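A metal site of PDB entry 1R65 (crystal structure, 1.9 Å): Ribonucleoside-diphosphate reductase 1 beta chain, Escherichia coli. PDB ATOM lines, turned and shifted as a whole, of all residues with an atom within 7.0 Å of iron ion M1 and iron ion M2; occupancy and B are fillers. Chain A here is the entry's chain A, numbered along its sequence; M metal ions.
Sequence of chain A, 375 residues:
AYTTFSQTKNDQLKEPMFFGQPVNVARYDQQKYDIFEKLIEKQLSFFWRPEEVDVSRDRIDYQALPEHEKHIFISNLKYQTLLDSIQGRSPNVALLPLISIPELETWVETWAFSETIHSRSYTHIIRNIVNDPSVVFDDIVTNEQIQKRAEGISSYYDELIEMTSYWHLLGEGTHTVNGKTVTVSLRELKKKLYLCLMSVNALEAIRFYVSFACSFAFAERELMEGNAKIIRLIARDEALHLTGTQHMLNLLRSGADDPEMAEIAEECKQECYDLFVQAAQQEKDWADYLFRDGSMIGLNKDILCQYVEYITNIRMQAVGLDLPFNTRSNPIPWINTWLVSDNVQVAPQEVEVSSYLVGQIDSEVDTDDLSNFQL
Merely in contact with iron ion M2: Phe 208 (3.7 Å). The nearest printed residue that does not touch iron ion M2 is Ile 234 (4.3 Å).
Trp 111 touches iron ion M1 (NE1 to FE, 3.6 Å). Within 4 Å of iron ion M1: Trp 111, Glu 115, Glu 204, Glu 238 and His 241.
Iron ion M1 is bound by the side-chain carboxylate (OE1) of Glu 238 (1.8 Å). OE2 of Glu 115 is bound to iron ion M1. ND1 of His 241 binds iron ion M1 (2.2 Å). Iron ion M1 has three donor atoms within binding distance. Slightly farther from iron ion M1 lies the side-chain carboxylate (OE1) of Glu 204 (2.6 Å). Slightly farther from iron ion M1 lies the side-chain carboxylate (OE2) of Glu 204 (2.7 Å). Slightly farther from iron ion M1 lies the side-chain carboxylate (OE2) of Glu 238 (2.8 Å).
The side-chain carboxylate (OD2) of Asp 84 lies within hydrogen-bond range of the side-chain hydroxyl (OH) of Tyr 122, 2.6 Å away. The backbone carbonyl oxygen (O) of Ser 114 lies close to a ring nitrogen (NE2) of His 118 (3.4 Å). The side-chain hydroxyl (OG) of Ser 119 is in hydrogen-bond range of the backbone carbonyl oxygen (O) of Glu 115, 3.4 Å away. A ring nitrogen (NE2) of His 241 is in hydrogen-bond range of the side-chain hydroxyl (OG) of Ser 114 (2.9 Å). The side-chain carboxylate of Glu 204 lies within hydrogen-bond range of the indole nitrogen of Trp 111, at 3.1 Å. The side-chain carboxylate of Glu 204 lies within hydrogen-bond range of the side-chain amide nitrogen of Gln 87 (3.3 Å). The backbone carbonyl oxygen (O) of Trp 111 lies within hydrogen-bond range of the side-chain hydroxyl (OG) of Ser 114. The backbone carbonyl oxygen (O) of Leu 203 lies within hydrogen-bond range of the backbone NH (N) of Phe 208 (3.2 Å).
The side-chain carboxylate (OD1) of Asp 84 is bound to iron ion M2. ND1 of His 118 binds iron ion M2 (2.1 Å). OE1 of Glu 115 is bound to iron ion M2 (2.1 Å). The side-chain carboxylate (OE2) of Glu 238 is bound to iron ion M2, 2.2 Å away.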
ATOM      1  N   GLN A  80      24.036  24.418 -21.222  1.00  0.00           N
ATOM      2  CA  GLN A  80      24.934  23.313 -21.575  1.00  0.00           C
ATOM      3  C   GLN A  80      26.149  23.333 -20.639  1.00  0.00           C
ATOM      4  O   GLN A  80      26.592  22.289 -20.164  1.00  0.00           O
ATOM      5  CB  GLN A  80      25.399  23.458 -23.054  1.00  0.00           C
ATOM      6  CG  GLN A  80      24.243  23.438 -24.076  1.00  0.00           C
ATOM      7  CD  GLN A  80      24.695  23.691 -25.523  1.00  0.00           C
ATOM      8  OE1 GLN A  80      25.480  24.594 -25.787  1.00  0.00           O
ATOM      9  NE2 GLN A  80      24.181  22.886 -26.441  1.00  0.00           N
ATOM     10  N   LEU A  83      25.046  21.761 -17.338  1.00  0.00           N
ATOM     11  CA  LEU A  83      24.897  20.324 -17.396  1.00  0.00           C
ATOM     12  C   LEU A  83      26.241  19.601 -17.388  1.00  0.00           C
ATOM     13  O   LEU A  83      26.414  18.624 -16.661  1.00  0.00           O
ATOM     14  CB  LEU A  83      24.097  19.910 -18.632  1.00  0.00           C
ATOM     15  CG  LEU A  83      22.615  20.306 -18.681  1.00  0.00           C
ATOM     16  CD1 LEU A  83      22.016  19.808 -19.989  1.00  0.00           C
ATOM     17  CD2 LEU A  83      21.873  19.709 -17.497  1.00  0.00           C
ATOM     18  N   ASP A  84      27.197  20.082 -18.171  1.00  0.00           N
ATOM     19  CA  ASP A  84      28.501  19.439 -18.199  1.00  0.00           C
ATOM     20  C   ASP A  84      29.338  19.709 -16.957  1.00  0.00           C
ATOM     21  O   ASP A  84      30.220  18.912 -16.618  1.00  0.00           O
ATOM     22  CB  ASP A  84      29.251  19.796 -19.486  1.00  0.00           C
ATOM     23  CG  ASP A  84      28.834  18.912 -20.658  1.00  0.00           C
ATOM     24  OD1 ASP A  84      28.842  17.680 -20.462  1.00  0.00           O
ATOM     25  OD2 ASP A  84      28.500  19.415 -21.750  1.00  0.00           O
ATOM     26  N   GLN A  87      27.996  17.050 -14.772  1.00  0.00           N
ATOM     27  CA  GLN A  87      28.346  15.733 -15.297  1.00  0.00           C
ATOM     28  C   GLN A  87      29.841  15.429 -15.303  1.00  0.00           C
ATOM     29  O   GLN A  87      30.240  14.294 -15.528  1.00  0.00           O
ATOM     30  CB  GLN A  87      27.786  15.561 -16.706  1.00  0.00           C
ATOM     31  CG  GLN A  87      26.264  15.400 -16.770  1.00  0.00           C
ATOM     32  CD  GLN A  87      25.763  14.227 -15.933  1.00  0.00           C
ATOM     33  OE1 GLN A  87      25.463  14.378 -14.741  1.00  0.00           O
ATOM     34  NE2 GLN A  87      25.671  13.057 -16.546  1.00  0.00           N
ATOM     35  N   TRP A 111      33.665   8.458 -19.023  1.00  0.00           N
ATOM     36  CA  TRP A 111      32.486   9.240 -19.332  1.00  0.00           C
ATOM     37  C   TRP A 111      32.612  10.620 -18.657  1.00  0.00           C
ATOM     38  O   TRP A 111      32.438  11.659 -19.313  1.00  0.00           O
ATOM     39  CB  TRP A 111      31.255   8.439 -18.845  1.00  0.00           C
ATOM     40  CG  TRP A 111      29.946   9.127 -18.722  1.00  0.00           C
ATOM     41  CD1 TRP A 111      29.538  10.265 -19.362  1.00  0.00           C
ATOM     42  CD2 TRP A 111      28.833   8.682 -17.948  1.00  0.00           C
ATOM     43  NE1 TRP A 111      28.232  10.535 -19.041  1.00  0.00           N
ATOM     44  CE2 TRP A 111      27.769   9.586 -18.175  1.00  0.00           C
ATOM     45  CE3 TRP A 111      28.621   7.593 -17.091  1.00  0.00           C
ATOM     46  CZ2 TRP A 111      26.518   9.436 -17.570  1.00  0.00           C
ATOM     47  CZ3 TRP A 111      27.369   7.443 -16.485  1.00  0.00           C
ATOM     48  CH2 TRP A 111      26.339   8.360 -16.733  1.00  0.00           C
ATOM     49  N   SER A 114      35.272  12.775 -20.343  1.00  0.00           N
ATOM     50  CA  SER A 114      34.820  13.378 -21.591  1.00  0.00           C
ATOM     51  C   SER A 114      33.961  14.612 -21.307  1.00  0.00           C
ATOM     52  O   SER A 114      33.931  15.542 -22.107  1.00  0.00           O
ATOM     53  CB  SER A 114      34.039  12.368 -22.447  1.00  0.00           C
ATOM     54  OG  SER A 114      32.738  12.127 -21.933  1.00  0.00           O
ATOM     55  N   GLU A 115      33.271  14.632 -20.176  1.00  0.00           N
ATOM     56  CA  GLU A 115      32.451  15.797 -19.847  1.00  0.00           C
ATOM     57  C   GLU A 115      33.339  16.993 -19.510  1.00  0.00           C
ATOM     58  O   GLU A 115      32.956  18.145 -19.764  1.00  0.00           O
ATOM     59  CB  GLU A 115      31.487  15.496 -18.687  1.00  0.00           C
ATOM     60  CG  GLU A 115      30.557  14.280 -18.913  1.00  0.00           C
ATOM     61  CD  GLU A 115      29.520  14.491 -20.014  1.00  0.00           C
ATOM     62  OE1 GLU A 115      29.862  15.027 -21.077  1.00  0.00           O
ATOM     63  OE2 GLU A 115      28.356  14.095 -19.830  1.00  0.00           O
ATOM     64  N   THR A 116      34.524  16.757 -18.942  1.00  0.00           N
ATOM     65  CA  THR A 116      35.406  17.891 -18.615  1.00  0.00           C
ATOM     66  C   THR A 116      35.929  18.505 -19.911  1.00  0.00           C
ATOM     67  O   THR A 116      36.187  19.699 -19.968  1.00  0.00           O
ATOM     68  CB  THR A 116      36.618  17.498 -17.726  1.00  0.00           C
ATOM     69  OG1 THR A 116      37.463  16.560 -18.424  1.00  0.00           O
ATOM     70  CG2 THR A 116      36.127  16.903 -16.421  1.00  0.00           C
ATOM     71  N   HIS A 118      34.148  18.706 -22.551  1.00  0.00           N
ATOM     72  CA  HIS A 118      33.013  19.492 -23.010  1.00  0.00           C
ATOM     73  C   HIS A 118      33.022  20.838 -22.299  1.00  0.00           C
ATOM     74  O   HIS A 118      32.795  21.890 -22.910  1.00  0.00           O
ATOM     75  CB  HIS A 118      31.708  18.747 -22.741  1.00  0.00           C
ATOM     76  CG  HIS A 118      31.590  17.465 -23.511  1.00  0.00           C
ATOM     77  ND1 HIS A 118      30.552  16.576 -23.331  1.00  0.00           N
ATOM     78  CD2 HIS A 118      32.395  16.921 -24.458  1.00  0.00           C
ATOM     79  CE1 HIS A 118      30.722  15.543 -24.128  1.00  0.00           C
ATOM     80  NE2 HIS A 118      31.832  15.717 -24.819  1.00  0.00           N
ATOM     81  N   SER A 119      33.293  20.832 -20.996  1.00  0.00           N
ATOM     82  CA  SER A 119      33.357  22.080 -20.225  1.00  0.00           C
ATOM     83  C   SER A 119      34.469  22.956 -20.773  1.00  0.00           C
ATOM     84  O   SER A 119      34.312  24.174 -20.898  1.00  0.00           O
ATOM     85  CB  SER A 119      33.604  21.787 -18.747  1.00  0.00           C
ATOM     86  OG  SER A 119      32.500  21.117 -18.180  1.00  0.00           O
ATOM     87  N   TYR A 122      33.310  24.835 -23.855  1.00  0.00           N
ATOM     88  CA  TYR A 122      32.428  25.980 -23.629  1.00  0.00           C
ATOM     89  C   TYR A 122      33.244  27.210 -23.252  1.00  0.00           C
ATOM     90  O   TYR A 122      32.878  28.336 -23.602  1.00  0.00           O
ATOM     91  CB  TYR A 122      31.392  25.706 -22.540  1.00  0.00           C
ATOM     92  CG  TYR A 122      30.512  24.516 -22.837  1.00  0.00           C
ATOM     93  CD1 TYR A 122      29.959  24.333 -24.112  1.00  0.00           C
ATOM     94  CD2 TYR A 122      30.240  23.551 -21.873  1.00  0.00           C
ATOM     95  CE1 TYR A 122      29.176  23.213 -24.412  1.00  0.00           C
ATOM     96  CE2 TYR A 122      29.456  22.434 -22.154  1.00  0.00           C
ATOM     97  CZ  TYR A 122      28.935  22.280 -23.420  1.00  0.00           C
ATOM     98  OH  TYR A 122      28.171  21.159 -23.708  1.00  0.00           O
ATOM     99  N   LEU A 203      18.623  13.181 -18.607  1.00  0.00           N
ATOM    100  CA  LEU A 203      19.494  14.319 -18.800  1.00  0.00           C
ATOM    101  C   LEU A 203      20.258  14.140 -20.122  1.00  0.00           C
ATOM    102  O   LEU A 203      20.320  15.044 -20.962  1.00  0.00           O
ATOM    103  CB  LEU A 203      20.474  14.431 -17.623  1.00  0.00           C
ATOM    104  CG  LEU A 203      21.487  15.576 -17.602  1.00  0.00           C
ATOM    105  CD1 LEU A 203      22.093  15.689 -16.212  1.00  0.00           C
ATOM    106  CD2 LEU A 203      22.570  15.334 -18.636  1.00  0.00           C
ATOM    107  N   GLU A 204      20.828  12.956 -20.285  1.00  0.00           N
ATOM    108  CA  GLU A 204      21.603  12.613 -21.470  1.00  0.00           C
ATOM    109  C   GLU A 204      20.765  12.512 -22.739  1.00  0.00           C
ATOM    110  O   GLU A 204      21.153  13.014 -23.793  1.00  0.00           O
ATOM    111  CB  GLU A 204      22.314  11.267 -21.250  1.00  0.00           C
ATOM    112  CG  GLU A 204      23.336  11.246 -20.120  1.00  0.00           C
ATOM    113  CD  GLU A 204      24.635  11.912 -20.509  1.00  0.00           C
ATOM    114  OE1 GLU A 204      24.754  12.346 -21.665  1.00  0.00           O
ATOM    115  OE2 GLU A 204      25.541  12.005 -19.650  1.00  0.00           O
ATOM    116  N   PHE A 208      20.064  17.324 -23.162  1.00  0.00           N
ATOM    117  CA  PHE A 208      21.143  17.668 -24.096  1.00  0.00           C
ATOM    118  C   PHE A 208      20.679  17.836 -25.541  1.00  0.00           C
ATOM    119  O   PHE A 208      21.112  18.765 -26.223  1.00  0.00           O
ATOM    120  CB  PHE A 208      22.261  16.629 -24.046  1.00  0.00           C
ATOM    121  CG  PHE A 208      23.349  16.944 -23.065  1.00  0.00           C
ATOM    122  CD1 PHE A 208      24.085  18.130 -23.175  1.00  0.00           C
ATOM    123  CD2 PHE A 208      23.653  16.072 -22.019  1.00  0.00           C
ATOM    124  CE1 PHE A 208      25.098  18.432 -22.269  1.00  0.00           C
ATOM    125  CE2 PHE A 208      24.664  16.364 -21.112  1.00  0.00           C
ATOM    126  CZ  PHE A 208      25.393  17.559 -21.234  1.00  0.00           C
ATOM    127  N   PHE A 212      20.879  20.879 -28.293  1.00  0.00           N
ATOM    128  CA  PHE A 212      21.580  20.734 -29.566  1.00  0.00           C
ATOM    129  C   PHE A 212      20.779  21.407 -30.670  1.00  0.00           C
ATOM    130  O   PHE A 212      21.337  22.081 -31.535  1.00  0.00           O
ATOM    131  CB  PHE A 212      21.791  19.261 -29.945  1.00  0.00           C
ATOM    132  CG  PHE A 212      22.681  18.515 -28.994  1.00  0.00           C
ATOM    133  CD1 PHE A 212      23.585  19.180 -28.185  1.00  0.00           C
ATOM    134  CD2 PHE A 212      22.615  17.118 -28.930  1.00  0.00           C
ATOM    135  CE1 PHE A 212      24.416  18.479 -27.317  1.00  0.00           C
ATOM    136  CE2 PHE A 212      23.446  16.406 -28.070  1.00  0.00           C
ATOM    137  CZ  PHE A 212      24.352  17.090 -27.264  1.00  0.00           C
ATOM    138  N   ILE A 234      30.461  17.094 -29.361  1.00  0.00           N
ATOM    139  CA  ILE A 234      29.854  16.876 -28.065  1.00  0.00           C
ATOM    140  C   ILE A 234      28.661  15.935 -28.213  1.00  0.00           C
ATOM    141  O   ILE A 234      28.509  15.003 -27.417  1.00  0.00           O
ATOM    142  CB  ILE A 234      29.383  18.203 -27.419  1.00  0.00           C
ATOM    143  CG1 ILE A 234      30.607  19.002 -26.982  1.00  0.00           C
ATOM    144  CG2 ILE A 234      28.468  17.921 -26.228  1.00  0.00           C
ATOM    145  CD1 ILE A 234      30.252  20.324 -26.285  1.00  0.00           C
ATOM    146  N   ASP A 237      29.610  12.395 -28.418  1.00  0.00           N
ATOM    147  CA  ASP A 237      29.936  11.804 -27.111  1.00  0.00           C
ATOM    148  C   ASP A 237      28.680  11.480 -26.305  1.00  0.00           C
ATOM    149  O   ASP A 237      28.572  10.417 -25.678  1.00  0.00           O
ATOM    150  CB  ASP A 237      30.815  12.759 -26.279  1.00  0.00           C
ATOM    151  CG  ASP A 237      32.217  12.939 -26.856  1.00  0.00           C
ATOM    152  OD1 ASP A 237      32.722  12.027 -27.555  1.00  0.00           O
ATOM    153  OD2 ASP A 237      32.832  13.985 -26.557  1.00  0.00           O
ATOM    154  N   GLU A 238      27.727  12.408 -26.295  1.00  0.00           N
ATOM    155  CA  GLU A 238      26.488  12.206 -25.548  1.00  0.00           C
ATOM    156  C   GLU A 238      25.731  10.964 -26.030  1.00  0.00           C
ATOM    157  O   GLU A 238      25.099  10.287 -25.241  1.00  0.00           O
ATOM    158  CB  GLU A 238      25.573  13.428 -25.652  1.00  0.00           C
ATOM    159  CG  GLU A 238      26.103  14.691 -24.988  1.00  0.00           C
ATOM    160  CD  GLU A 238      26.820  14.404 -23.677  1.00  0.00           C
ATOM    161  OE1 GLU A 238      26.288  13.628 -22.865  1.00  0.00           O
ATOM    162  OE2 GLU A 238      27.900  14.963 -23.447  1.00  0.00           O
ATOM    163  N   ALA A 239      25.797  10.692 -27.323  1.00  0.00           N
ATOM    164  CA  ALA A 239      25.114   9.524 -27.872  1.00  0.00           C
ATOM    165  C   ALA A 239      25.703   8.252 -27.247  1.00  0.00           C
ATOM    166  O   ALA A 239      24.985   7.276 -27.017  1.00  0.00           O
ATOM    167  CB  ALA A 239      25.272   9.482 -29.386  1.00  0.00           C
ATOM    168  N   HIS A 241      27.148   8.196 -24.219  1.00  0.00           N
ATOM    169  CA  HIS A 241      26.751   8.264 -22.830  1.00  0.00           C
ATOM    170  C   HIS A 241      25.334   7.754 -22.637  1.00  0.00           C
ATOM    171  O   HIS A 241      25.074   6.986 -21.713  1.00  0.00           O
ATOM    172  CB  HIS A 241      26.869   9.712 -22.319  1.00  0.00           C
ATOM    173  CG  HIS A 241      28.237  10.286 -22.454  1.00  0.00           C
ATOM    174  ND1 HIS A 241      28.534  11.600 -22.162  1.00  0.00           N
ATOM    175  CD2 HIS A 241      29.412   9.722 -22.861  1.00  0.00           C
ATOM    176  CE1 HIS A 241      29.816  11.827 -22.371  1.00  0.00           C
ATOM    177  NE2 HIS A 241      30.366  10.707 -22.799  1.00  0.00           N
ATOM    178  N   LEU A 242      24.416   8.181 -23.499  1.00  0.00           N
ATOM    179  CA  LEU A 242      23.038   7.733 -23.344  1.00  0.00           C
ATOM    180  C   LEU A 242      22.918   6.245 -23.655  1.00  0.00           C
ATOM    181  O   LEU A 242      22.082   5.535 -23.091  1.00  0.00           O
ATOM    182  CB  LEU A 242      22.088   8.558 -24.220  1.00  0.00           C
ATOM    183  CG  LEU A 242      21.713   8.179 -25.652  1.00  0.00           C
ATOM    184  CD1 LEU A 242      20.907   6.893 -25.654  1.00  0.00           C
ATOM    185  CD2 LEU A 242      20.875   9.298 -26.252  1.00  0.00           C
HETATM  186 FE    FE M   1      27.232  13.163 -21.355  1.00  0.00          FE
HETATM  187 FE    FE M   2      28.803  16.535 -22.152  1.00  0.00          FE
